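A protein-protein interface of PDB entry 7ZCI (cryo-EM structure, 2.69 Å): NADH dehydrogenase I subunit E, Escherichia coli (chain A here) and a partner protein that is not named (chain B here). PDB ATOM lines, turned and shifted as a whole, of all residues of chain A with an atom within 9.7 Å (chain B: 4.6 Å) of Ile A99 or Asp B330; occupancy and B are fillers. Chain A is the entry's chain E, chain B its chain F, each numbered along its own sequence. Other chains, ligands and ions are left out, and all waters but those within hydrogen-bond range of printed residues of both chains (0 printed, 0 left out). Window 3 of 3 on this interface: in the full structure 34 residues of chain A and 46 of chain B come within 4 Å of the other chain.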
ATOM      1  N   CYS A  92      -2.769  22.620  31.657  1.00  0.00           N
ATOM      2  CA  CYS A  92      -1.373  22.501  31.277  1.00  0.00           C
ATOM      3  C   CYS A  92      -0.921  23.692  30.447  1.00  0.00           C
ATOM      4  O   CYS A  92      -1.621  24.147  29.540  1.00  0.00           O
ATOM      5  CB  CYS A  92      -1.133  21.219  30.502  1.00  0.00           C
ATOM      6  SG  CYS A  92       0.588  21.015  30.108  1.00  0.00           S
ATOM      7  N   ASP A  93       0.278  24.172  30.752  1.00  0.00           N
ATOM      8  CA  ASP A  93       0.846  25.368  30.156  1.00  0.00           C
ATOM      9  C   ASP A  93       1.974  25.069  29.188  1.00  0.00           C
ATOM     10  O   ASP A  93       2.391  25.965  28.453  1.00  0.00           O
ATOM     11  CB  ASP A  93       1.385  26.281  31.268  1.00  0.00           C
ATOM     12  CG  ASP A  93       1.006  27.714  31.087  1.00  0.00           C
ATOM     13  OD1 ASP A  93      -0.005  27.975  30.421  1.00  0.00           O
ATOM     14  OD2 ASP A  93       1.714  28.583  31.632  1.00  0.00           O
ATOM     15  N   SER A  94       2.471  23.839  29.165  1.00  0.00           N
ATOM     16  CA  SER A  94       3.747  23.525  28.544  1.00  0.00           C
ATOM     17  C   SER A  94       3.593  23.349  27.036  1.00  0.00           C
ATOM     18  O   SER A  94       2.554  23.647  26.447  1.00  0.00           O
ATOM     19  CB  SER A  94       4.363  22.303  29.208  1.00  0.00           C
ATOM     20  OG  SER A  94       4.640  22.561  30.568  1.00  0.00           O
ATOM     21  N   VAL A  95       4.644  22.832  26.403  1.00  0.00           N
ATOM     22  CA  VAL A  95       4.889  23.101  24.993  1.00  0.00           C
ATOM     23  C   VAL A  95       4.040  22.211  24.087  1.00  0.00           C
ATOM     24  O   VAL A  95       3.565  22.661  23.039  1.00  0.00           O
ATOM     25  CB  VAL A  95       6.400  22.976  24.709  1.00  0.00           C
ATOM     26  CG1 VAL A  95       6.943  21.601  25.071  1.00  0.00           C
ATOM     27  CG2 VAL A  95       6.725  23.339  23.294  1.00  0.00           C
ATOM     28  N   VAL A  96       3.811  20.955  24.471  1.00  0.00           N
ATOM     29  CA  VAL A  96       2.993  20.074  23.645  1.00  0.00           C
ATOM     30  C   VAL A  96       1.535  20.508  23.681  1.00  0.00           C
ATOM     31  O   VAL A  96       0.838  20.467  22.664  1.00  0.00           O
ATOM     32  CB  VAL A  96       3.163  18.610  24.082  1.00  0.00           C
ATOM     33  CG1 VAL A  96       2.577  17.684  23.046  1.00  0.00           C
ATOM     34  CG2 VAL A  96       4.622  18.297  24.293  1.00  0.00           C
ATOM     35  N   CYS A  97       1.050  20.937  24.847  1.00  0.00           N
ATOM     36  CA  CYS A  97      -0.294  21.489  24.916  1.00  0.00           C
ATOM     37  C   CYS A  97      -0.370  22.872  24.293  1.00  0.00           C
ATOM     38  O   CYS A  97      -1.461  23.317  23.932  1.00  0.00           O
ATOM     39  CB  CYS A  97      -0.778  21.532  26.363  1.00  0.00           C
ATOM     40  SG  CYS A  97      -0.966  19.909  27.119  1.00  0.00           S
ATOM     41  N   HIS A  98       0.761  23.566  24.167  1.00  0.00           N
ATOM     42  CA  HIS A  98       0.786  24.796  23.390  1.00  0.00           C
ATOM     43  C   HIS A  98       0.604  24.507  21.910  1.00  0.00           C
ATOM     44  O   HIS A  98      -0.113  25.232  21.215  1.00  0.00           O
ATOM     45  CB  HIS A  98       2.092  25.546  23.636  1.00  0.00           C
ATOM     46  CG  HIS A  98       2.228  26.801  22.834  1.00  0.00           C
ATOM     47  ND1 HIS A  98       2.833  26.831  21.598  1.00  0.00           N
ATOM     48  CD2 HIS A  98       1.840  28.071  23.095  1.00  0.00           C
ATOM     49  CE1 HIS A  98       2.811  28.065  21.130  1.00  0.00           C
ATOM     50  NE2 HIS A  98       2.215  28.837  22.019  1.00  0.00           N
ATOM     51  N   ILE A  99       1.247  23.451  21.412  1.00  0.00           N
ATOM     52  CA  ILE A  99       1.061  23.052  20.023  1.00  0.00           C
ATOM     53  C   ILE A  99      -0.356  22.537  19.797  1.00  0.00           C
ATOM     54  O   ILE A  99      -0.989  22.846  18.782  1.00  0.00           O
ATOM     55  CB  ILE A  99       2.123  22.012  19.629  1.00  0.00           C
ATOM     56  CG1 ILE A  99       3.507  22.631  19.748  1.00  0.00           C
ATOM     57  CG2 ILE A  99       1.927  21.547  18.220  1.00  0.00           C
ATOM     58  CD1 ILE A  99       4.609  21.736  19.321  1.00  0.00           C
ATOM     59  N   ASN A 100      -0.889  21.785  20.751  1.00  0.00           N
ATOM     60  CA  ASN A 100      -2.244  21.258  20.658  1.00  0.00           C
ATOM     61  C   ASN A 100      -3.308  22.293  20.993  1.00  0.00           C
ATOM     62  O   ASN A 100      -4.495  21.960  20.982  1.00  0.00           O
ATOM     63  CB  ASN A 100      -2.392  20.045  21.574  1.00  0.00           C
ATOM     64  CG  ASN A 100      -1.619  18.849  21.074  1.00  0.00           C
ATOM     65  OD1 ASN A 100      -1.632  18.544  19.886  1.00  0.00           O
ATOM     66  ND2 ASN A 100      -0.928  18.171  21.977  1.00  0.00           N
ATOM     67  N   GLY A 101      -2.919  23.526  21.301  1.00  0.00           N
ATOM     68  CA  GLY A 101      -3.875  24.595  21.483  1.00  0.00           C
ATOM     69  C   GLY A 101      -4.467  24.702  22.870  1.00  0.00           C
ATOM     70  O   GLY A 101      -5.689  24.643  23.024  1.00  0.00           O
ATOM     71  N   TYR A 102      -3.623  24.858  23.893  1.00  0.00           N
ATOM     72  CA  TYR A 102      -4.155  25.103  25.226  1.00  0.00           C
ATOM     73  C   TYR A 102      -4.737  26.500  25.362  1.00  0.00           C
ATOM     74  O   TYR A 102      -5.505  26.738  26.296  1.00  0.00           O
ATOM     75  CB  TYR A 102      -3.082  24.887  26.308  1.00  0.00           C
ATOM     76  CG  TYR A 102      -2.241  26.108  26.651  1.00  0.00           C
ATOM     77  CD1 TYR A 102      -1.088  26.389  25.944  1.00  0.00           C
ATOM     78  CD2 TYR A 102      -2.594  26.969  27.687  1.00  0.00           C
ATOM     79  CE1 TYR A 102      -0.318  27.485  26.240  1.00  0.00           C
ATOM     80  CE2 TYR A 102      -1.847  28.078  27.968  1.00  0.00           C
ATOM     81  CZ  TYR A 102      -0.700  28.325  27.252  1.00  0.00           C
ATOM     82  OH  TYR A 102       0.064  29.426  27.549  1.00  0.00           O
ATOM     83  N   GLN A 103      -4.355  27.433  24.484  1.00  0.00           N
ATOM     84  CA  GLN A 103      -4.801  28.815  24.622  1.00  0.00           C
ATOM     85  C   GLN A 103      -6.305  28.934  24.439  1.00  0.00           C
ATOM     86  O   GLN A 103      -6.949  29.750  25.106  1.00  0.00           O
ATOM     87  CB  GLN A 103      -4.074  29.712  23.626  1.00  0.00           C
ATOM     88  CG  GLN A 103      -2.692  30.135  24.067  1.00  0.00           C
ATOM     89  CD  GLN A 103      -1.604  29.558  23.200  1.00  0.00           C
ATOM     90  OE1 GLN A 103      -1.675  28.403  22.779  1.00  0.00           O
ATOM     91  NE2 GLN A 103      -0.588  30.362  22.919  1.00  0.00           N
ATOM     92  N   GLY A 104      -6.882  28.128  23.549  1.00  0.00           N
ATOM     93  CA  GLY A 104      -8.329  28.096  23.426  1.00  0.00           C
ATOM     94  C   GLY A 104      -9.004  27.585  24.683  1.00  0.00           C
ATOM     95  O   GLY A 104     -10.052  28.094  25.085  1.00  0.00           O
ATOM     96  N   CYS A 137       1.208  14.162  27.283  1.00  0.00           N
ATOM     97  CA  CYS A 137       1.391  15.037  26.134  1.00  0.00           C
ATOM     98  C   CYS A 137       0.832  14.441  24.852  1.00  0.00           C
ATOM     99  O   CYS A 137       0.464  15.186  23.940  1.00  0.00           O
ATOM    100  CB  CYS A 137       2.872  15.359  25.976  1.00  0.00           C
ATOM    101  SG  CYS A 137       3.666  15.751  27.530  1.00  0.00           S
ATOM    102  N   GLY A 140      -2.989  15.603  24.590  1.00  0.00           N
ATOM    103  CA  GLY A 140      -3.201  16.991  24.924  1.00  0.00           C
ATOM    104  C   GLY A 140      -4.296  17.628  24.101  1.00  0.00           C
ATOM    105  O   GLY A 140      -4.748  17.098  23.079  1.00  0.00           O
ATOM    106  N   PRO A 141      -4.750  18.811  24.544  1.00  0.00           N
ATOM    107  CA  PRO A 141      -4.371  19.533  25.764  1.00  0.00           C
ATOM    108  C   PRO A 141      -5.016  18.952  27.020  1.00  0.00           C
ATOM    109  O   PRO A 141      -6.046  18.296  26.935  1.00  0.00           O
ATOM    110  CB  PRO A 141      -4.862  20.955  25.491  1.00  0.00           C
ATOM    111  CG  PRO A 141      -5.969  20.792  24.553  1.00  0.00           C
ATOM    112  CD  PRO A 141      -5.645  19.613  23.696  1.00  0.00           C
ATOM    113  N   ARG B 255       0.455  17.012  17.155  1.00  0.00           N
ATOM    114  CA  ARG B 255      -0.151  17.207  15.831  1.00  0.00           C
ATOM    115  C   ARG B 255       0.332  16.185  14.808  1.00  0.00           C
ATOM    116  O   ARG B 255       0.541  16.499  13.638  1.00  0.00           O
ATOM    117  CB  ARG B 255       0.076  18.629  15.327  1.00  0.00           C
ATOM    118  CG  ARG B 255      -0.442  19.668  16.273  1.00  0.00           C
ATOM    119  CD  ARG B 255      -1.609  20.415  15.697  1.00  0.00           C
ATOM    120  NE  ARG B 255      -1.156  21.570  14.937  1.00  0.00           N
ATOM    121  CZ  ARG B 255      -1.842  22.696  14.810  1.00  0.00           C
ATOM    122  NH1 ARG B 255      -3.020  22.854  15.387  1.00  0.00           N
ATOM    123  NH2 ARG B 255      -1.331  23.688  14.088  1.00  0.00           N
ATOM    124  N   MET B 281       2.436  13.339   9.912  1.00  0.00           N
ATOM    125  CA  MET B 281       1.782  14.534  10.410  1.00  0.00           C
ATOM    126  C   MET B 281       0.300  14.504  10.053  1.00  0.00           C
ATOM    127  O   MET B 281      -0.143  13.737   9.197  1.00  0.00           O
ATOM    128  CB  MET B 281       2.460  15.778   9.850  1.00  0.00           C
ATOM    129  CG  MET B 281       3.895  15.895  10.304  1.00  0.00           C
ATOM    130  SD  MET B 281       4.020  16.480  11.993  1.00  0.00           S
ATOM    131  CE  MET B 281       3.826  18.221  11.739  1.00  0.00           C
ATOM    132  N   LEU B 285      -0.975  19.604   7.404  1.00  0.00           N
ATOM    133  CA  LEU B 285       0.109  20.101   8.236  1.00  0.00           C
ATOM    134  C   LEU B 285       1.439  19.676   7.639  1.00  0.00           C
ATOM    135  O   LEU B 285       1.583  18.549   7.158  1.00  0.00           O
ATOM    136  CB  LEU B 285      -0.003  19.588   9.671  1.00  0.00           C
ATOM    137  CG  LEU B 285      -1.155  20.146  10.499  1.00  0.00           C
ATOM    138  CD1 LEU B 285      -1.134  19.551  11.884  1.00  0.00           C
ATOM    139  CD2 LEU B 285      -1.065  21.652  10.568  1.00  0.00           C
ATOM    140  N   LYS B 286       2.405  20.585   7.669  1.00  0.00           N
ATOM    141  CA  LYS B 286       3.730  20.351   7.119  1.00  0.00           C
ATOM    142  C   LYS B 286       4.738  20.286   8.254  1.00  0.00           C
ATOM    143  O   LYS B 286       4.767  21.168   9.114  1.00  0.00           O
ATOM    144  CB  LYS B 286       4.110  21.451   6.128  1.00  0.00           C
ATOM    145  CG  LYS B 286       4.579  20.939   4.779  1.00  0.00           C
ATOM    146  CD  LYS B 286       3.563  19.996   4.157  1.00  0.00           C
ATOM    147  CE  LYS B 286       2.343  20.740   3.645  1.00  0.00           C
ATOM    148  NZ  LYS B 286       1.320  19.805   3.101  1.00  0.00           N
ATOM    149  N   LYS B 288       7.906  20.866  10.196  1.00  0.00           N
ATOM    150  CA  LYS B 288       8.939  21.889  10.134  1.00  0.00           C
ATOM    151  C   LYS B 288      10.069  21.693  11.133  1.00  0.00           C
ATOM    152  O   LYS B 288      11.194  22.090  10.831  1.00  0.00           O
ATOM    153  CB  LYS B 288       8.331  23.295  10.310  1.00  0.00           C
ATOM    154  CG  LYS B 288       8.311  23.847  11.715  1.00  0.00           C
ATOM    155  CD  LYS B 288       7.807  25.276  11.765  1.00  0.00           C
ATOM    156  CE  LYS B 288       8.791  26.263  11.195  1.00  0.00           C
ATOM    157  NZ  LYS B 288       8.302  27.649  11.416  1.00  0.00           N
ATOM    158  N   MET B 327       8.987  15.422  19.915  1.00  0.00           N
ATOM    159  CA  MET B 327       7.844  16.291  19.694  1.00  0.00           C
ATOM    160  C   MET B 327       7.980  16.930  18.323  1.00  0.00           C
ATOM    161  O   MET B 327       9.025  17.506  18.005  1.00  0.00           O
ATOM    162  CB  MET B 327       7.757  17.352  20.787  1.00  0.00           C
ATOM    163  CG  MET B 327       6.898  18.539  20.444  1.00  0.00           C
ATOM    164  SD  MET B 327       7.072  19.814  21.693  1.00  0.00           S
ATOM    165  CE  MET B 327       7.910  21.060  20.727  1.00  0.00           C
ATOM    166  N   ALA B 328       6.933  16.814  17.515  1.00  0.00           N
ATOM    167  CA  ALA B 328       6.921  17.327  16.153  1.00  0.00           C
ATOM    168  C   ALA B 328       6.268  18.698  16.115  1.00  0.00           C
ATOM    169  O   ALA B 328       5.239  18.927  16.755  1.00  0.00           O
ATOM    170  CB  ALA B 328       6.179  16.375  15.217  1.00  0.00           C
ATOM    171  N   VAL B 329       6.870  19.610  15.361  1.00  0.00           N
ATOM    172  CA  VAL B 329       6.401  20.979  15.228  1.00  0.00           C
ATOM    173  C   VAL B 329       6.028  21.209  13.775  1.00  0.00           C
ATOM    174  O   VAL B 329       6.876  21.061  12.883  1.00  0.00           O
ATOM    175  CB  VAL B 329       7.464  21.991  15.670  1.00  0.00           C
ATOM    176  CG1 VAL B 329       6.896  23.370  15.591  1.00  0.00           C
ATOM    177  CG2 VAL B 329       7.943  21.690  17.071  1.00  0.00           C
ATOM    178  N   ASP B 330       4.777  21.600  13.548  1.00  0.00           N
ATOM    179  CA  ASP B 330       4.239  21.886  12.229  1.00  0.00           C
ATOM    180  C   ASP B 330       4.510  23.329  11.818  1.00  0.00           C
ATOM    181  O   ASP B 330       4.888  24.175  12.627  1.00  0.00           O
ATOM    182  CB  ASP B 330       2.738  21.610  12.190  1.00  0.00           C
ATOM    183  CG  ASP B 330       2.004  22.231  13.351  1.00  0.00           C
ATOM    184  OD1 ASP B 330       2.421  22.003  14.502  1.00  0.00           O
ATOM    185  OD2 ASP B 330       1.009  22.944  13.115  1.00  0.00           O
ATOM    186  N   HIS B 331       4.277  23.604  10.532  1.00  0.00           N
ATOM    187  CA  HIS B 331       4.564  24.910   9.953  1.00  0.00           C
ATOM    188  C   HIS B 331       3.663  26.011  10.490  1.00  0.00           C
ATOM    189  O   HIS B 331       4.011  27.188  10.372  1.00  0.00           O
ATOM    190  CB  HIS B 331       4.428  24.848   8.436  1.00  0.00           C
ATOM    191  CG  HIS B 331       3.009  24.808   7.965  1.00  0.00           C
ATOM    192  ND1 HIS B 331       2.198  23.709   8.145  1.00  0.00           N
ATOM    193  CD2 HIS B 331       2.248  25.738   7.343  1.00  0.00           C
ATOM    194  CE1 HIS B 331       1.003  23.958   7.642  1.00  0.00           C
ATOM    195  NE2 HIS B 331       1.006  25.184   7.150  1.00  0.00           N
ATOM    196  N   GLU B 332       2.520  25.660  11.067  1.00  0.00           N
ATOM    197  CA  GLU B 332       1.603  26.641  11.625  1.00  0.00           C
ATOM    198  C   GLU B 332       2.043  27.147  12.990  1.00  0.00           C
ATOM    199  O   GLU B 332       1.394  28.044  13.541  1.00  0.00           O
ATOM    200  CB  GLU B 332       0.202  26.040  11.728  1.00  0.00           C
ATOM    201  CG  GLU B 332      -0.439  25.749  10.390  1.00  0.00           C
ATOM    202  CD  GLU B 332      -1.895  25.362  10.521  1.00  0.00           C
ATOM    203  OE1 GLU B 332      -2.426  25.420  11.648  1.00  0.00           O
ATOM    204  OE2 GLU B 332      -2.509  24.996   9.497  1.00  0.00           O
ATOM    205  N   ILE B 333       3.113  26.595  13.547  1.00  0.00           N
ATOM    206  CA  ILE B 333       3.620  26.984  14.854  1.00  0.00           C
ATOM    207  C   ILE B 333       4.752  27.977  14.647  1.00  0.00           C
ATOM    208  O   ILE B 333       5.722  27.688  13.937  1.00  0.00           O
ATOM    209  CB  ILE B 333       4.096  25.760  15.651  1.00  0.00           C
ATOM    210  CG1 ILE B 333       2.911  24.872  16.019  1.00  0.00           C
ATOM    211  CG2 ILE B 333       4.844  26.193  16.895  1.00  0.00           C
ATOM    212  CD1 ILE B 333       1.881  25.558  16.866  1.00  0.00           C
ATOM    213  N   LEU B 338       6.830  29.419  20.434  1.00  0.00           N
ATOM    214  CA  LEU B 338       7.162  28.133  21.039  1.00  0.00           C
ATOM    215  C   LEU B 338       8.329  28.257  22.008  1.00  0.00           C
ATOM    216  O   LEU B 338       8.292  27.717  23.119  1.00  0.00           O
ATOM    217  CB  LEU B 338       7.486  27.112  19.956  1.00  0.00           C
ATOM    218  CG  LEU B 338       7.240  25.686  20.423  1.00  0.00           C
ATOM    219  CD1 LEU B 338       5.755  25.455  20.478  1.00  0.00           C
ATOM    220  CD2 LEU B 338       7.900  24.685  19.518  1.00  0.00           C
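CE of Met B327 touches CG2 of Val A95, 3.6 Å away. Val A95 touches Leu B338. CG2 of Val A96 touches SD of Met B327, at 3.9 Å. His A98 touches Leu B338 (ND1 to CD1, 3.4 Å). CG2 of Ile A99 touches CG of Arg B255 (3.6 Å). Met B327 touches Ile A99. CD1 of Ile A99 touches O of Ala B328, 3.9 Å away. CG2 of Ile A99 touches OD1 of Asp B330, 3.8 Å away. CG1 of Ile A99 touches CD1 of Leu B338, 3.7 Å away. Asn A100 touches Arg B255.
Of the printed residues of chain B, Val A96 touches Met B327 (3.9 Å). Of the printed residues of chain A, Met B327 touches Val A95, Val A96 and Ile A99. No residue of chain A comes within 4 Å of Val B329. Asp B330 touches just one residue of chain A: Ile A99 (3.8 Å). No residue of chain A comes within 4 Å of Glu B332. No residue of chain A comes within 4 Å of Ile B333. The nearest residue of chain B that does not touch Ile A99 is Val B329 (4.02 Å).
Along chain A the printed residues that touch a printed residue of chain B span positions 95 to 100. Among the printed residues, 10 pairs touch across the chains. Among the printed residues, no Asp or Glu carboxylate lies within 4 Å of a Lys or Arg side-chain nitrogen of the other chain.
OE1 of Glu B332 is in salt-bridge range of NH2 of Arg B255 (3.2 Å). The guanidinium group (NH2) of Arg B255 lies within salt-bridge range of the side-chain carboxylate (OD2) of Asp B330 (2.6 Å). The backbone carbonyl oxygen (O) of Val A96 lies within hydrogen-bond range of the side-chain amide nitrogen (ND2) of Asn A100 (3.0 Å). NE2 of Gln A103 lies within hydrogen-bond range of NE2 of His A98 (3.3 Å).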
